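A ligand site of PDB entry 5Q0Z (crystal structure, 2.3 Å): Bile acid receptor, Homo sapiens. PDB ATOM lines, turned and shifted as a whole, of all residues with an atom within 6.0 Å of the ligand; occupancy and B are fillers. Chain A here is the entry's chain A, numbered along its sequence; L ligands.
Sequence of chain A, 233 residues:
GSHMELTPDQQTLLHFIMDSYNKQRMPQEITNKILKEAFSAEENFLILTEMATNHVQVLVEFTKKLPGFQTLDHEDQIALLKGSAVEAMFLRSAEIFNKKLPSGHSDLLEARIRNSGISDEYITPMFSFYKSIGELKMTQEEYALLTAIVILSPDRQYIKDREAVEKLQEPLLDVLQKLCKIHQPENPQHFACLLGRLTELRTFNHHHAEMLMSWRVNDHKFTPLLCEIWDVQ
The backbone carbonyl oxygen of Leu 48 sits at hydrogen-bond distance from a nitrogen (N2) of the ligand (3.2 Å). The side-chain hydroxyl (OG) of Ser 93 sits close to an oxygen (O1) of the ligand, 3.3 Å away. The backbone NH (N) of Ala 52 is in hydrogen-bond range of an oxygen (O2) of the ligand. The side-chain hydroxyl (OH) of Tyr 130 is in hydrogen-bond range of an oxygen (O3) of the ligand (3.2 Å).
The backbone carbonyl oxygen (O) of Thr 49 lies within hydrogen-bond range of the side-chain hydroxyl (OG1) of Thr 53. O of Ile 113 lies within hydrogen-bond range of OG of Ser 116 (2.7 Å). The backbone carbonyl oxygen of Tyr 130 lies within hydrogen-bond range of the side-chain amide nitrogen of Asn 98, at 2.8 Å. The side-chain hydroxyl (OG1) of Thr 49 lies within hydrogen-bond range of the backbone carbonyl oxygen (O) of Phe 45 (2.9 Å). The side-chain hydroxyl (OH) of Tyr 130 lies close to the side-chain sulfur (SD) of Met 126 (3.8 Å). OG1 of Thr 31 sits at hydrogen-bond distance from O of Pro 27 (3.0 Å). O of Ser 116 is in hydrogen-bond range of NE1 of Trp 215, 3.1 Å away. OG of Ser 93 sits at hydrogen-bond distance from O of Met 89, 2.7 Å away.
The backbone NH (N) of Phe 97 sits close to a fluorine (F2) of the ligand (3.2 Å). Ile 30 touches the ligand (CG2 to F1, 3.3 Å). Thr 31 touches the ligand. Ile 34 touches the ligand. N of Thr 49 touches C19 of the ligand (3.8 Å). Met 51 touches the ligand. His 55 touches the ligand (CB to C12, 3.9 Å). CG of Met 89 touches O1 of the ligand, at 3.6 Å. CE1 of Phe 90 touches C17 of the ligand (3.9 Å). CG of Arg 92 touches C13 of the ligand, 3.8 Å away. Ile 96 touches the ligand. CD2 of Leu 109 touches F2 of the ligand (3.6 Å). Ile 113 touches the ligand (CD1 to C24, 3.7 Å). CE of Met 126 touches C17 of the ligand, 3.7 Å away. Met 211 touches the ligand (CE to C17, 3.7 Å). Leu 212 touches the ligand (CD2 to C21, 3.5 Å). Trp 215 touches the ligand (CZ3 to C11, 3.5 Å). CH2 of Trp 230 touches C19 of the ligand, at 3.9 Å. Hydrophobic or aromatic side chains within 4 Å of the ligand: Ile 30, Ile 34, Leu 48, Met 51, Ala 52, His 55, Met 89, Phe 90, Ile 96, Phe 97, Leu 109, Ile 113, Met 126, Tyr 130, Met 211, Leu 212, Trp 215 and Trp 230. Of the 33 residues printed, 22 come within 4 Å of the ligand. The nearest printed residue that does not touch the ligand is Phe 45 (4.2 Å).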
ATOM      1  N   PRO A  27      -8.884 -15.475  -9.354  1.00  0.00           N
ATOM      2  CA  PRO A  27      -8.062 -16.543  -8.753  1.00  0.00           C
ATOM      3  C   PRO A  27      -6.613 -16.516  -9.239  1.00  0.00           C
ATOM      4  O   PRO A  27      -5.713 -16.825  -8.448  1.00  0.00           O
ATOM      5  CB  PRO A  27      -8.779 -17.826  -9.198  1.00  0.00           C
ATOM      6  CG  PRO A  27     -10.173 -17.423  -9.437  1.00  0.00           C
ATOM      7  CD  PRO A  27     -10.081 -16.042 -10.016  1.00  0.00           C
ATOM      8  N   ILE A  30      -4.371 -14.059  -7.302  1.00  0.00           N
ATOM      9  CA  ILE A  30      -3.968 -14.626  -6.010  1.00  0.00           C
ATOM     10  C   ILE A  30      -2.903 -15.726  -6.202  1.00  0.00           C
ATOM     11  O   ILE A  30      -1.883 -15.706  -5.524  1.00  0.00           O
ATOM     12  CB  ILE A  30      -5.228 -15.078  -5.207  1.00  0.00           C
ATOM     13  CG1 ILE A  30      -5.910 -13.865  -4.555  1.00  0.00           C
ATOM     14  CG2 ILE A  30      -4.919 -16.163  -4.159  1.00  0.00           C
ATOM     15  CD1 ILE A  30      -7.383 -13.877  -4.640  1.00  0.00           C
ATOM     16  N   THR A  31      -3.133 -16.681  -7.133  1.00  0.00           N
ATOM     17  CA  THR A  31      -2.200 -17.782  -7.402  1.00  0.00           C
ATOM     18  C   THR A  31      -0.868 -17.338  -8.012  1.00  0.00           C
ATOM     19  O   THR A  31       0.161 -17.923  -7.664  1.00  0.00           O
ATOM     20  CB  THR A  31      -2.845 -18.901  -8.249  1.00  0.00           C
ATOM     21  OG1 THR A  31      -3.388 -18.363  -9.447  1.00  0.00           O
ATOM     22  CG2 THR A  31      -3.895 -19.673  -7.489  1.00  0.00           C
ATOM     23  N   ILE A  34       1.704 -16.081  -5.197  1.00  0.00           N
ATOM     24  CA  ILE A  34       2.234 -17.211  -4.417  1.00  0.00           C
ATOM     25  C   ILE A  34       3.208 -18.058  -5.249  1.00  0.00           C
ATOM     26  O   ILE A  34       4.320 -18.335  -4.791  1.00  0.00           O
ATOM     27  CB  ILE A  34       1.086 -18.043  -3.781  1.00  0.00           C
ATOM     28  CG1 ILE A  34       0.052 -17.131  -3.059  1.00  0.00           C
ATOM     29  CG2 ILE A  34       1.636 -19.112  -2.818  1.00  0.00           C
ATOM     30  CD1 ILE A  34      -1.301 -17.738  -2.891  1.00  0.00           C
ATOM     31  N   PHE A  45       2.632 -14.108   5.638  1.00  0.00           N
ATOM     32  CA  PHE A  45       1.620 -13.618   6.573  1.00  0.00           C
ATOM     33  C   PHE A  45       1.107 -12.242   6.139  1.00  0.00           C
ATOM     34  O   PHE A  45      -0.079 -11.960   6.283  1.00  0.00           O
ATOM     35  CB  PHE A  45       2.153 -13.573   8.010  1.00  0.00           C
ATOM     36  CG  PHE A  45       1.079 -13.331   9.057  1.00  0.00           C
ATOM     37  CD1 PHE A  45       0.260 -14.370   9.484  1.00  0.00           C
ATOM     38  CD2 PHE A  45       0.926 -12.080   9.645  1.00  0.00           C
ATOM     39  CE1 PHE A  45      -0.727 -14.158  10.449  1.00  0.00           C
ATOM     40  CE2 PHE A  45      -0.060 -11.869  10.620  1.00  0.00           C
ATOM     41  CZ  PHE A  45      -0.873 -12.903  11.016  1.00  0.00           C
ATOM     42  N   LEU A  48      -0.992 -12.851   2.830  1.00  0.00           N
ATOM     43  CA  LEU A  48      -2.268 -13.444   3.202  1.00  0.00           C
ATOM     44  C   LEU A  48      -3.191 -12.472   3.976  1.00  0.00           C
ATOM     45  O   LEU A  48      -4.404 -12.511   3.771  1.00  0.00           O
ATOM     46  CB  LEU A  48      -2.064 -14.785   3.953  1.00  0.00           C
ATOM     47  CG  LEU A  48      -1.459 -15.963   3.140  1.00  0.00           C
ATOM     48  CD1 LEU A  48      -1.044 -17.088   4.054  1.00  0.00           C
ATOM     49  CD2 LEU A  48      -2.417 -16.496   2.092  1.00  0.00           C
ATOM     50  N   THR A  49      -2.608 -11.593   4.834  1.00  0.00           N
ATOM     51  CA  THR A  49      -3.334 -10.549   5.581  1.00  0.00           C
ATOM     52  C   THR A  49      -3.989  -9.552   4.595  1.00  0.00           C
ATOM     53  O   THR A  49      -5.153  -9.194   4.782  1.00  0.00           O
ATOM     54  CB  THR A  49      -2.431  -9.899   6.653  1.00  0.00           C
ATOM     55  OG1 THR A  49      -2.293 -10.828   7.730  1.00  0.00           O
ATOM     56  CG2 THR A  49      -2.984  -8.586   7.207  1.00  0.00           C
ATOM     57  N   MET A  51      -4.626 -10.199   1.318  1.00  0.00           N
ATOM     58  CA  MET A  51      -5.575 -11.019   0.563  1.00  0.00           C
ATOM     59  C   MET A  51      -6.891 -11.095   1.324  1.00  0.00           C
ATOM     60  O   MET A  51      -7.937 -10.829   0.747  1.00  0.00           O
ATOM     61  CB  MET A  51      -5.048 -12.447   0.378  1.00  0.00           C
ATOM     62  CG  MET A  51      -4.162 -12.628  -0.797  1.00  0.00           C
ATOM     63  SD  MET A  51      -3.759 -14.383  -1.019  1.00  0.00           S
ATOM     64  CE  MET A  51      -2.419 -14.222  -2.161  1.00  0.00           C
ATOM     65  N   ALA A  52      -6.834 -11.420   2.628  1.00  0.00           N
ATOM     66  CA  ALA A  52      -8.018 -11.520   3.494  1.00  0.00           C
ATOM     67  C   ALA A  52      -8.731 -10.192   3.714  1.00  0.00           C
ATOM     68  O   ALA A  52      -9.955 -10.194   3.754  1.00  0.00           O
ATOM     69  CB  ALA A  52      -7.641 -12.129   4.817  1.00  0.00           C
ATOM     70  N   THR A  53      -7.981  -9.070   3.854  1.00  0.00           N
ATOM     71  CA  THR A  53      -8.547  -7.724   4.018  1.00  0.00           C
ATOM     72  C   THR A  53      -9.344  -7.372   2.755  1.00  0.00           C
ATOM     73  O   THR A  53     -10.484  -6.906   2.876  1.00  0.00           O
ATOM     74  CB  THR A  53      -7.461  -6.687   4.349  1.00  0.00           C
ATOM     75  OG1 THR A  53      -6.753  -7.120   5.516  1.00  0.00           O
ATOM     76  CG2 THR A  53      -8.030  -5.300   4.617  1.00  0.00           C
ATOM     77  N   HIS A  55     -10.569  -9.578   0.603  1.00  0.00           N
ATOM     78  CA  HIS A  55     -11.690 -10.518   0.575  1.00  0.00           C
ATOM     79  C   HIS A  55     -12.874  -9.983   1.380  1.00  0.00           C
ATOM     80  O   HIS A  55     -13.987  -9.961   0.856  1.00  0.00           O
ATOM     81  CB  HIS A  55     -11.306 -11.937   1.060  1.00  0.00           C
ATOM     82  CG  HIS A  55     -12.499 -12.837   1.062  1.00  0.00           C
ATOM     83  ND1 HIS A  55     -13.254 -13.024   2.210  1.00  0.00           N
ATOM     84  CD2 HIS A  55     -13.111 -13.468   0.031  1.00  0.00           C
ATOM     85  CE1 HIS A  55     -14.274 -13.775   1.839  1.00  0.00           C
ATOM     86  NE2 HIS A  55     -14.219 -14.088   0.544  1.00  0.00           N
ATOM     87  N   MET A  89     -14.566 -16.906   3.238  1.00  0.00           N
ATOM     88  CA  MET A  89     -13.149 -16.878   2.856  1.00  0.00           C
ATOM     89  C   MET A  89     -12.641 -18.287   2.523  1.00  0.00           C
ATOM     90  O   MET A  89     -11.918 -18.430   1.540  1.00  0.00           O
ATOM     91  CB  MET A  89     -12.272 -16.213   3.922  1.00  0.00           C
ATOM     92  CG  MET A  89     -10.849 -15.955   3.463  1.00  0.00           C
ATOM     93  SD  MET A  89      -9.651 -15.648   4.784  1.00  0.00           S
ATOM     94  CE  MET A  89      -9.500 -17.313   5.471  1.00  0.00           C
ATOM     95  N   PHE A  90     -13.034 -19.316   3.308  1.00  0.00           N
ATOM     96  CA  PHE A  90     -12.649 -20.709   3.069  1.00  0.00           C
ATOM     97  C   PHE A  90     -13.353 -21.297   1.849  1.00  0.00           C
ATOM     98  O   PHE A  90     -12.750 -22.098   1.140  1.00  0.00           O
ATOM     99  CB  PHE A  90     -12.828 -21.581   4.314  1.00  0.00           C
ATOM    100  CG  PHE A  90     -11.710 -21.342   5.317  1.00  0.00           C
ATOM    101  CD1 PHE A  90     -10.432 -21.874   5.107  1.00  0.00           C
ATOM    102  CD2 PHE A  90     -11.930 -20.572   6.457  1.00  0.00           C
ATOM    103  CE1 PHE A  90      -9.395 -21.639   6.018  1.00  0.00           C
ATOM    104  CE2 PHE A  90     -10.879 -20.344   7.376  1.00  0.00           C
ATOM    105  CZ  PHE A  90      -9.622 -20.881   7.147  1.00  0.00           C
ATOM    106  N   ARG A  92     -14.213 -19.428  -0.815  1.00  0.00           N
ATOM    107  CA  ARG A  92     -13.486 -18.762  -1.910  1.00  0.00           C
ATOM    108  C   ARG A  92     -12.094 -19.386  -2.108  1.00  0.00           C
ATOM    109  O   ARG A  92     -11.699 -19.633  -3.244  1.00  0.00           O
ATOM    110  CB  ARG A  92     -13.396 -17.247  -1.695  1.00  0.00           C
ATOM    111  CG  ARG A  92     -12.683 -16.468  -2.811  1.00  0.00           C
ATOM    112  CD  ARG A  92     -13.370 -16.535  -4.162  1.00  0.00           C
ATOM    113  NE  ARG A  92     -12.591 -15.849  -5.201  1.00  0.00           N
ATOM    114  CZ  ARG A  92     -12.920 -15.796  -6.482  1.00  0.00           C
ATOM    115  NH1 ARG A  92     -14.014 -16.395  -6.926  1.00  0.00           N
ATOM    116  NH2 ARG A  92     -12.147 -15.139  -7.341  1.00  0.00           N
ATOM    117  N   SER A  93     -11.369 -19.651  -1.003  1.00  0.00           N
ATOM    118  CA  SER A  93     -10.037 -20.277  -1.043  1.00  0.00           C
ATOM    119  C   SER A  93     -10.105 -21.649  -1.706  1.00  0.00           C
ATOM    120  O   SER A  93      -9.185 -22.019  -2.432  1.00  0.00           O
ATOM    121  CB  SER A  93      -9.474 -20.408   0.359  1.00  0.00           C
ATOM    122  OG  SER A  93      -9.372 -19.134   0.951  1.00  0.00           O
ATOM    123  N   ALA A  94     -11.199 -22.396  -1.473  1.00  0.00           N
ATOM    124  CA  ALA A  94     -11.445 -23.714  -2.052  1.00  0.00           C
ATOM    125  C   ALA A  94     -11.627 -23.585  -3.556  1.00  0.00           C
ATOM    126  O   ALA A  94     -11.063 -24.374  -4.301  1.00  0.00           O
ATOM    127  CB  ALA A  94     -12.686 -24.343  -1.414  1.00  0.00           C
ATOM    128  N   ILE A  96     -10.457 -21.123  -5.525  1.00  0.00           N
ATOM    129  CA  ILE A  96      -9.150 -20.754  -6.085  1.00  0.00           C
ATOM    130  C   ILE A  96      -8.228 -21.977  -6.199  1.00  0.00           C
ATOM    131  O   ILE A  96      -7.677 -22.204  -7.280  1.00  0.00           O
ATOM    132  CB  ILE A  96      -8.498 -19.574  -5.306  1.00  0.00           C
ATOM    133  CG1 ILE A  96      -9.421 -18.334  -5.272  1.00  0.00           C
ATOM    134  CG2 ILE A  96      -7.143 -19.207  -5.923  1.00  0.00           C
ATOM    135  CD1 ILE A  96      -9.022 -17.253  -4.250  1.00  0.00           C
ATOM    136  N   PHE A  97      -8.061 -22.762  -5.127  1.00  0.00           N
ATOM    137  CA  PHE A  97      -7.197 -23.939  -5.132  1.00  0.00           C
ATOM    138  C   PHE A  97      -7.589 -24.984  -6.182  1.00  0.00           C
ATOM    139  O   PHE A  97      -6.708 -25.573  -6.817  1.00  0.00           O
ATOM    140  CB  PHE A  97      -7.096 -24.585  -3.732  1.00  0.00           C
ATOM    141  CG  PHE A  97      -6.187 -25.786  -3.672  1.00  0.00           C
ATOM    142  CD1 PHE A  97      -4.805 -25.644  -3.811  1.00  0.00           C
ATOM    143  CD2 PHE A  97      -6.701 -27.068  -3.484  1.00  0.00           C
ATOM    144  CE1 PHE A  97      -3.964 -26.768  -3.780  1.00  0.00           C
ATOM    145  CE2 PHE A  97      -5.851 -28.181  -3.433  1.00  0.00           C
ATOM    146  CZ  PHE A  97      -4.495 -28.025  -3.579  1.00  0.00           C
ATOM    147  N   ASN A  98      -8.903 -25.201  -6.367  1.00  0.00           N
ATOM    148  CA  ASN A  98      -9.441 -26.184  -7.317  1.00  0.00           C
ATOM    149  C   ASN A  98      -9.471 -25.720  -8.777  1.00  0.00           C
ATOM    150  O   ASN A  98      -9.791 -26.540  -9.660  1.00  0.00           O
ATOM    151  CB  ASN A  98     -10.820 -26.659  -6.866  1.00  0.00           C
ATOM    152  CG  ASN A  98     -10.745 -27.547  -5.650  1.00  0.00           C
ATOM    153  OD1 ASN A  98     -10.109 -28.593  -5.652  1.00  0.00           O
ATOM    154  ND2 ASN A  98     -11.415 -27.144  -4.596  1.00  0.00           N
ATOM    155  N   LEU A 109       1.394 -24.819  -5.402  1.00  0.00           N
ATOM    156  CA  LEU A 109       0.586 -23.876  -4.622  1.00  0.00           C
ATOM    157  C   LEU A 109       0.302 -24.468  -3.238  1.00  0.00           C
ATOM    158  O   LEU A 109       0.434 -23.757  -2.241  1.00  0.00           O
ATOM    159  CB  LEU A 109      -0.720 -23.526  -5.357  1.00  0.00           C
ATOM    160  CG  LEU A 109      -1.682 -22.548  -4.650  1.00  0.00           C
ATOM    161  CD1 LEU A 109      -1.182 -21.115  -4.715  1.00  0.00           C
ATOM    162  CD2 LEU A 109      -3.077 -22.648  -5.232  1.00  0.00           C
ATOM    163  N   ILE A 113       1.686 -22.932   0.538  1.00  0.00           N
ATOM    164  CA  ILE A 113       0.718 -22.651   1.606  1.00  0.00           C
ATOM    165  C   ILE A 113       1.072 -23.480   2.857  1.00  0.00           C
ATOM    166  O   ILE A 113       1.065 -22.936   3.959  1.00  0.00           O
ATOM    167  CB  ILE A 113      -0.764 -22.850   1.138  1.00  0.00           C
ATOM    168  CG1 ILE A 113      -1.129 -21.847   0.010  1.00  0.00           C
ATOM    169  CG2 ILE A 113      -1.750 -22.719   2.310  1.00  0.00           C
ATOM    170  CD1 ILE A 113      -2.322 -22.246  -0.864  1.00  0.00           C
ATOM    171  N   SER A 116       4.022 -21.843   4.617  1.00  0.00           N
ATOM    172  CA  SER A 116       3.852 -20.397   4.745  1.00  0.00           C
ATOM    173  C   SER A 116       3.950 -19.855   6.199  1.00  0.00           C
ATOM    174  O   SER A 116       3.887 -18.635   6.392  1.00  0.00           O
ATOM    175  CB  SER A 116       2.551 -19.938   4.087  1.00  0.00           C
ATOM    176  OG  SER A 116       1.422 -20.395   4.814  1.00  0.00           O
ATOM    177  N   ILE A 118       2.057 -21.436   8.873  1.00  0.00           N
ATOM    178  CA  ILE A 118       0.897 -22.044   9.545  1.00  0.00           C
ATOM    179  C   ILE A 118       1.225 -23.418  10.160  1.00  0.00           C
ATOM    180  O   ILE A 118       2.023 -24.164   9.595  1.00  0.00           O
ATOM    181  CB  ILE A 118      -0.305 -22.078   8.543  1.00  0.00           C
ATOM    182  CG1 ILE A 118      -1.578 -22.746   9.162  1.00  0.00           C
ATOM    183  CG2 ILE A 118       0.074 -22.675   7.185  1.00  0.00           C
ATOM    184  CD1 ILE A 118      -2.883 -22.469   8.422  1.00  0.00           C
ATOM    185  N   MET A 126      -7.888 -28.256   6.293  1.00  0.00           N
ATOM    186  CA  MET A 126      -8.080 -27.195   5.311  1.00  0.00           C
ATOM    187  C   MET A 126      -7.924 -27.737   3.881  1.00  0.00           C
ATOM    188  O   MET A 126      -8.826 -27.531   3.063  1.00  0.00           O
ATOM    189  CB  MET A 126      -7.068 -26.069   5.575  1.00  0.00           C
ATOM    190  CG  MET A 126      -7.521 -24.725   5.112  1.00  0.00           C
ATOM    191  SD  MET A 126      -6.210 -23.528   5.459  1.00  0.00           S
ATOM    192  CE  MET A 126      -6.367 -23.388   7.258  1.00  0.00           C
ATOM    193  N   PHE A 127      -6.793 -28.430   3.585  1.00  0.00           N
ATOM    194  CA  PHE A 127      -6.561 -29.022   2.254  1.00  0.00           C
ATOM    195  C   PHE A 127      -7.438 -30.236   2.021  1.00  0.00           C
ATOM    196  O   PHE A 127      -7.700 -30.571   0.859  1.00  0.00           O
ATOM    197  CB  PHE A 127      -5.071 -29.305   1.976  1.00  0.00           C
ATOM    198  CG  PHE A 127      -4.336 -28.077   1.490  1.00  0.00           C
ATOM    199  CD1 PHE A 127      -4.574 -27.567   0.217  1.00  0.00           C
ATOM    200  CD2 PHE A 127      -3.424 -27.430   2.298  1.00  0.00           C
ATOM    201  CE1 PHE A 127      -3.915 -26.417  -0.226  1.00  0.00           C
ATOM    202  CE2 PHE A 127      -2.756 -26.277   1.855  1.00  0.00           C
ATOM    203  CZ  PHE A 127      -3.009 -25.784   0.592  1.00  0.00           C
ATOM    204  N   TYR A 130     -10.655 -28.530   0.870  1.00  0.00           N
ATOM    205  CA  TYR A 130     -10.448 -28.026  -0.502  1.00  0.00           C
ATOM    206  C   TYR A 130     -10.525 -29.159  -1.511  1.00  0.00           C
ATOM    207  O   TYR A 130     -11.169 -29.002  -2.551  1.00  0.00           O
ATOM    208  CB  TYR A 130      -9.106 -27.276  -0.650  1.00  0.00           C
ATOM    209  CG  TYR A 130      -8.906 -26.039   0.201  1.00  0.00           C
ATOM    210  CD1 TYR A 130      -9.976 -25.412   0.839  1.00  0.00           C
ATOM    211  CD2 TYR A 130      -7.646 -25.456   0.334  1.00  0.00           C
ATOM    212  CE1 TYR A 130      -9.792 -24.279   1.625  1.00  0.00           C
ATOM    213  CE2 TYR A 130      -7.454 -24.318   1.100  1.00  0.00           C
ATOM    214  CZ  TYR A 130      -8.534 -23.726   1.746  1.00  0.00           C
ATOM    215  OH  TYR A 130      -8.337 -22.608   2.509  1.00  0.00           O
ATOM    216  N   HIS A 208     -10.256 -20.381  14.431  1.00  0.00           N
ATOM    217  CA  HIS A 208      -9.683 -19.448  13.460  1.00  0.00           C
ATOM    218  C   HIS A 208      -8.641 -18.493  14.072  1.00  0.00           C
ATOM    219  O   HIS A 208      -7.509 -18.456  13.590  1.00  0.00           O
ATOM    220  CB  HIS A 208     -10.776 -18.667  12.709  1.00  0.00           C
ATOM    221  CG  HIS A 208     -10.243 -17.856  11.573  1.00  0.00           C
ATOM    222  ND1 HIS A 208      -9.719 -18.453  10.442  1.00  0.00           N
ATOM    223  CD2 HIS A 208     -10.164 -16.510  11.436  1.00  0.00           C
ATOM    224  CE1 HIS A 208      -9.337 -17.458   9.657  1.00  0.00           C
ATOM    225  NE2 HIS A 208      -9.591 -16.266  10.211  1.00  0.00           N
ATOM    226  N   MET A 211      -5.476 -20.305  14.971  1.00  0.00           N
ATOM    227  CA  MET A 211      -4.657 -20.611  13.796  1.00  0.00           C
ATOM    228  C   MET A 211      -3.794 -19.387  13.437  1.00  0.00           C
ATOM    229  O   MET A 211      -2.598 -19.529  13.169  1.00  0.00           O
ATOM    230  CB  MET A 211      -5.577 -21.059  12.638  1.00  0.00           C
ATOM    231  CG  MET A 211      -4.871 -21.215  11.293  1.00  0.00           C
ATOM    232  SD  MET A 211      -4.702 -19.681  10.332  1.00  0.00           S
ATOM    233  CE  MET A 211      -6.391 -19.407   9.865  1.00  0.00           C
ATOM    234  N   LEU A 212      -4.414 -18.180  13.457  1.00  0.00           N
ATOM    235  CA  LEU A 212      -3.761 -16.901  13.174  1.00  0.00           C
ATOM    236  C   LEU A 212      -2.648 -16.579  14.173  1.00  0.00           C
ATOM    237  O   LEU A 212      -1.583 -16.137  13.743  1.00  0.00           O
ATOM    238  CB  LEU A 212      -4.786 -15.758  13.143  1.00  0.00           C
ATOM    239  CG  LEU A 212      -5.977 -15.877  12.195  1.00  0.00           C
ATOM    240  CD1 LEU A 212      -7.069 -14.909  12.584  1.00  0.00           C
ATOM    241  CD2 LEU A 212      -5.554 -15.688  10.741  1.00  0.00           C
ATOM    242  N   TRP A 215       0.724 -18.811  14.177  1.00  0.00           N
ATOM    243  CA  TRP A 215       1.524 -18.617  12.974  1.00  0.00           C
ATOM    244  C   TRP A 215       2.971 -18.391  13.387  1.00  0.00           C
ATOM    245  O   TRP A 215       3.232 -17.605  14.315  1.00  0.00           O
ATOM    246  CB  TRP A 215       1.018 -17.404  12.177  1.00  0.00           C
ATOM    247  CG  TRP A 215       1.367 -17.456  10.715  1.00  0.00           C
ATOM    248  CD1 TRP A 215       2.533 -17.043  10.132  1.00  0.00           C
ATOM    249  CD2 TRP A 215       0.550 -17.968   9.663  1.00  0.00           C
ATOM    250  NE1 TRP A 215       2.484 -17.275   8.773  1.00  0.00           N
ATOM    251  CE2 TRP A 215       1.271 -17.827   8.456  1.00  0.00           C
ATOM    252  CE3 TRP A 215      -0.739 -18.536   9.615  1.00  0.00           C
ATOM    253  CZ2 TRP A 215       0.751 -18.233   7.217  1.00  0.00           C
ATOM    254  CZ3 TRP A 215      -1.258 -18.911   8.388  1.00  0.00           C
ATOM    255  CH2 TRP A 215      -0.508 -18.786   7.207  1.00  0.00           C
ATOM    256  N   PHE A 222      -2.222  -7.363  12.007  1.00  0.00           N
ATOM    257  CA  PHE A 222      -3.443  -7.443  11.207  1.00  0.00           C
ATOM    258  C   PHE A 222      -3.953  -6.038  10.915  1.00  0.00           C
ATOM    259  O   PHE A 222      -3.650  -5.096  11.666  1.00  0.00           O
ATOM    260  CB  PHE A 222      -4.546  -8.219  11.952  1.00  0.00           C
ATOM    261  CG  PHE A 222      -4.215  -9.626  12.363  1.00  0.00           C
ATOM    262  CD1 PHE A 222      -4.386 -10.694  11.479  1.00  0.00           C
ATOM    263  CD2 PHE A 222      -3.792  -9.915  13.660  1.00  0.00           C
ATOM    264  CE1 PHE A 222      -4.108 -12.000  11.872  1.00  0.00           C
ATOM    265  CE2 PHE A 222      -3.511 -11.230  14.053  1.00  0.00           C
ATOM    266  CZ  PHE A 222      -3.664 -12.259  13.149  1.00  0.00           C
ATOM    267  N   LEU A 226      -9.708  -6.486   9.681  1.00  0.00           N
ATOM    268  CA  LEU A 226      -9.546  -7.898  10.059  1.00  0.00           C
ATOM    269  C   LEU A 226      -9.734  -8.085  11.559  1.00  0.00           C
ATOM    270  O   LEU A 226     -10.408  -9.025  11.956  1.00  0.00           O
ATOM    271  CB  LEU A 226      -8.191  -8.470   9.627  1.00  0.00           C
ATOM    272  CG  LEU A 226      -8.043  -8.928   8.172  1.00  0.00           C
ATOM    273  CD1 LEU A 226      -6.663  -9.522   7.947  1.00  0.00           C
ATOM    274  CD2 LEU A 226      -9.108  -9.943   7.790  1.00  0.00           C
ATOM    275  N   TRP A 230     -12.547 -10.681  12.527  1.00  0.00           N
ATOM    276  CA  TRP A 230     -11.984 -11.908  13.106  1.00  0.00           C
ATOM    277  C   TRP A 230     -11.867 -11.913  14.645  1.00  0.00           C
ATOM    278  O   TRP A 230     -11.532 -12.945  15.210  1.00  0.00           O
ATOM    279  CB  TRP A 230     -10.612 -12.215  12.476  1.00  0.00           C
ATOM    280  CG  TRP A 230     -10.645 -12.656  11.041  1.00  0.00           C
ATOM    281  CD1 TRP A 230     -11.736 -13.039  10.319  1.00  0.00           C
ATOM    282  CD2 TRP A 230      -9.512 -12.835  10.183  1.00  0.00           C
ATOM    283  NE1 TRP A 230     -11.355 -13.414   9.055  1.00  0.00           N
ATOM    284  CE2 TRP A 230      -9.989 -13.311   8.945  1.00  0.00           C
ATOM    285  CE3 TRP A 230      -8.125 -12.624  10.340  1.00  0.00           C
ATOM    286  CZ2 TRP A 230      -9.133 -13.605   7.878  1.00  0.00           C
ATOM    287  CZ3 TRP A 230      -7.286 -12.924   9.284  1.00  0.00           C
ATOM    288  CH2 TRP A 230      -7.786 -13.421   8.078  1.00  0.00           C
HETATM  289  N1  LIG L   1      -6.234 -19.354   2.435  1.00  0.00           N
HETATM  290  C1  LIG L   1      -5.373 -17.669   4.966  1.00  0.00           C
HETATM  291  C2  LIG L   1      -6.550 -18.035   2.006  1.00  0.00           C
HETATM  292  C3  LIG L   1      -5.446 -19.242   4.856  1.00  0.00           C
HETATM  293  C4  LIG L   1      -5.682 -20.344   1.569  1.00  0.00           C
HETATM  294  C5  LIG L   1      -4.932 -15.477   5.679  1.00  0.00           C
HETATM  295  C6  LIG L   1      -5.370 -20.064   0.132  1.00  0.00           C
HETATM  296  C7  LIG L   1      -5.457 -20.745  -2.148  1.00  0.00           C
HETATM  297  C8  LIG L   1      -4.791 -19.600  -2.521  1.00  0.00           C
HETATM  298  C9  LIG L   1      -4.405 -18.672  -1.588  1.00  0.00           C
HETATM  299  C10 LIG L   1      -4.056 -19.825   4.550  1.00  0.00           C
HETATM  300  C11 LIG L   1      -3.991 -17.120   7.190  1.00  0.00           C
HETATM  301  C12 LIG L   1      -8.920 -14.945   0.396  1.00  0.00           C
HETATM  302  C13 LIG L   1      -9.650 -15.527  -0.740  1.00  0.00           C
HETATM  303  O1  LIG L   1      -8.164 -16.075   1.112  1.00  0.00           O
HETATM  304  C14 LIG L   1      -7.264 -15.728   2.055  1.00  0.00           C
HETATM  305  O2  LIG L   1      -6.942 -14.594   2.272  1.00  0.00           O
HETATM  306  C15 LIG L   1      -6.728 -16.925   2.779  1.00  0.00           C
HETATM  307  C16 LIG L   1      -6.498 -19.732   3.840  1.00  0.00           C
HETATM  308  C17 LIG L   1      -5.898 -19.848   6.197  1.00  0.00           C
HETATM  309  C18 LIG L   1      -5.972 -16.678   4.003  1.00  0.00           C
HETATM  310  N2  LIG L   1      -5.663 -15.385   4.494  1.00  0.00           N
HETATM  311  C19 LIG L   1      -4.431 -14.450   6.485  1.00  0.00           C
HETATM  312  C20 LIG L   1      -3.719 -14.764   7.629  1.00  0.00           C
HETATM  313  C21 LIG L   1      -3.501 -16.094   7.976  1.00  0.00           C
HETATM  314  C22 LIG L   1      -4.718 -16.829   6.026  1.00  0.00           C
HETATM  315  O3  LIG L   1      -5.440 -21.454   1.998  1.00  0.00           O
HETATM  316  C23 LIG L   1      -4.686 -18.912  -0.253  1.00  0.00           C
HETATM  317  F1  LIG L   1      -4.521 -19.386  -3.837  1.00  0.00           F
HETATM  318  F2  LIG L   1      -5.827 -21.625  -3.100  1.00  0.00           F
HETATM  319  C24 LIG L   1      -5.756 -21.000  -0.832  1.00  0.00           C
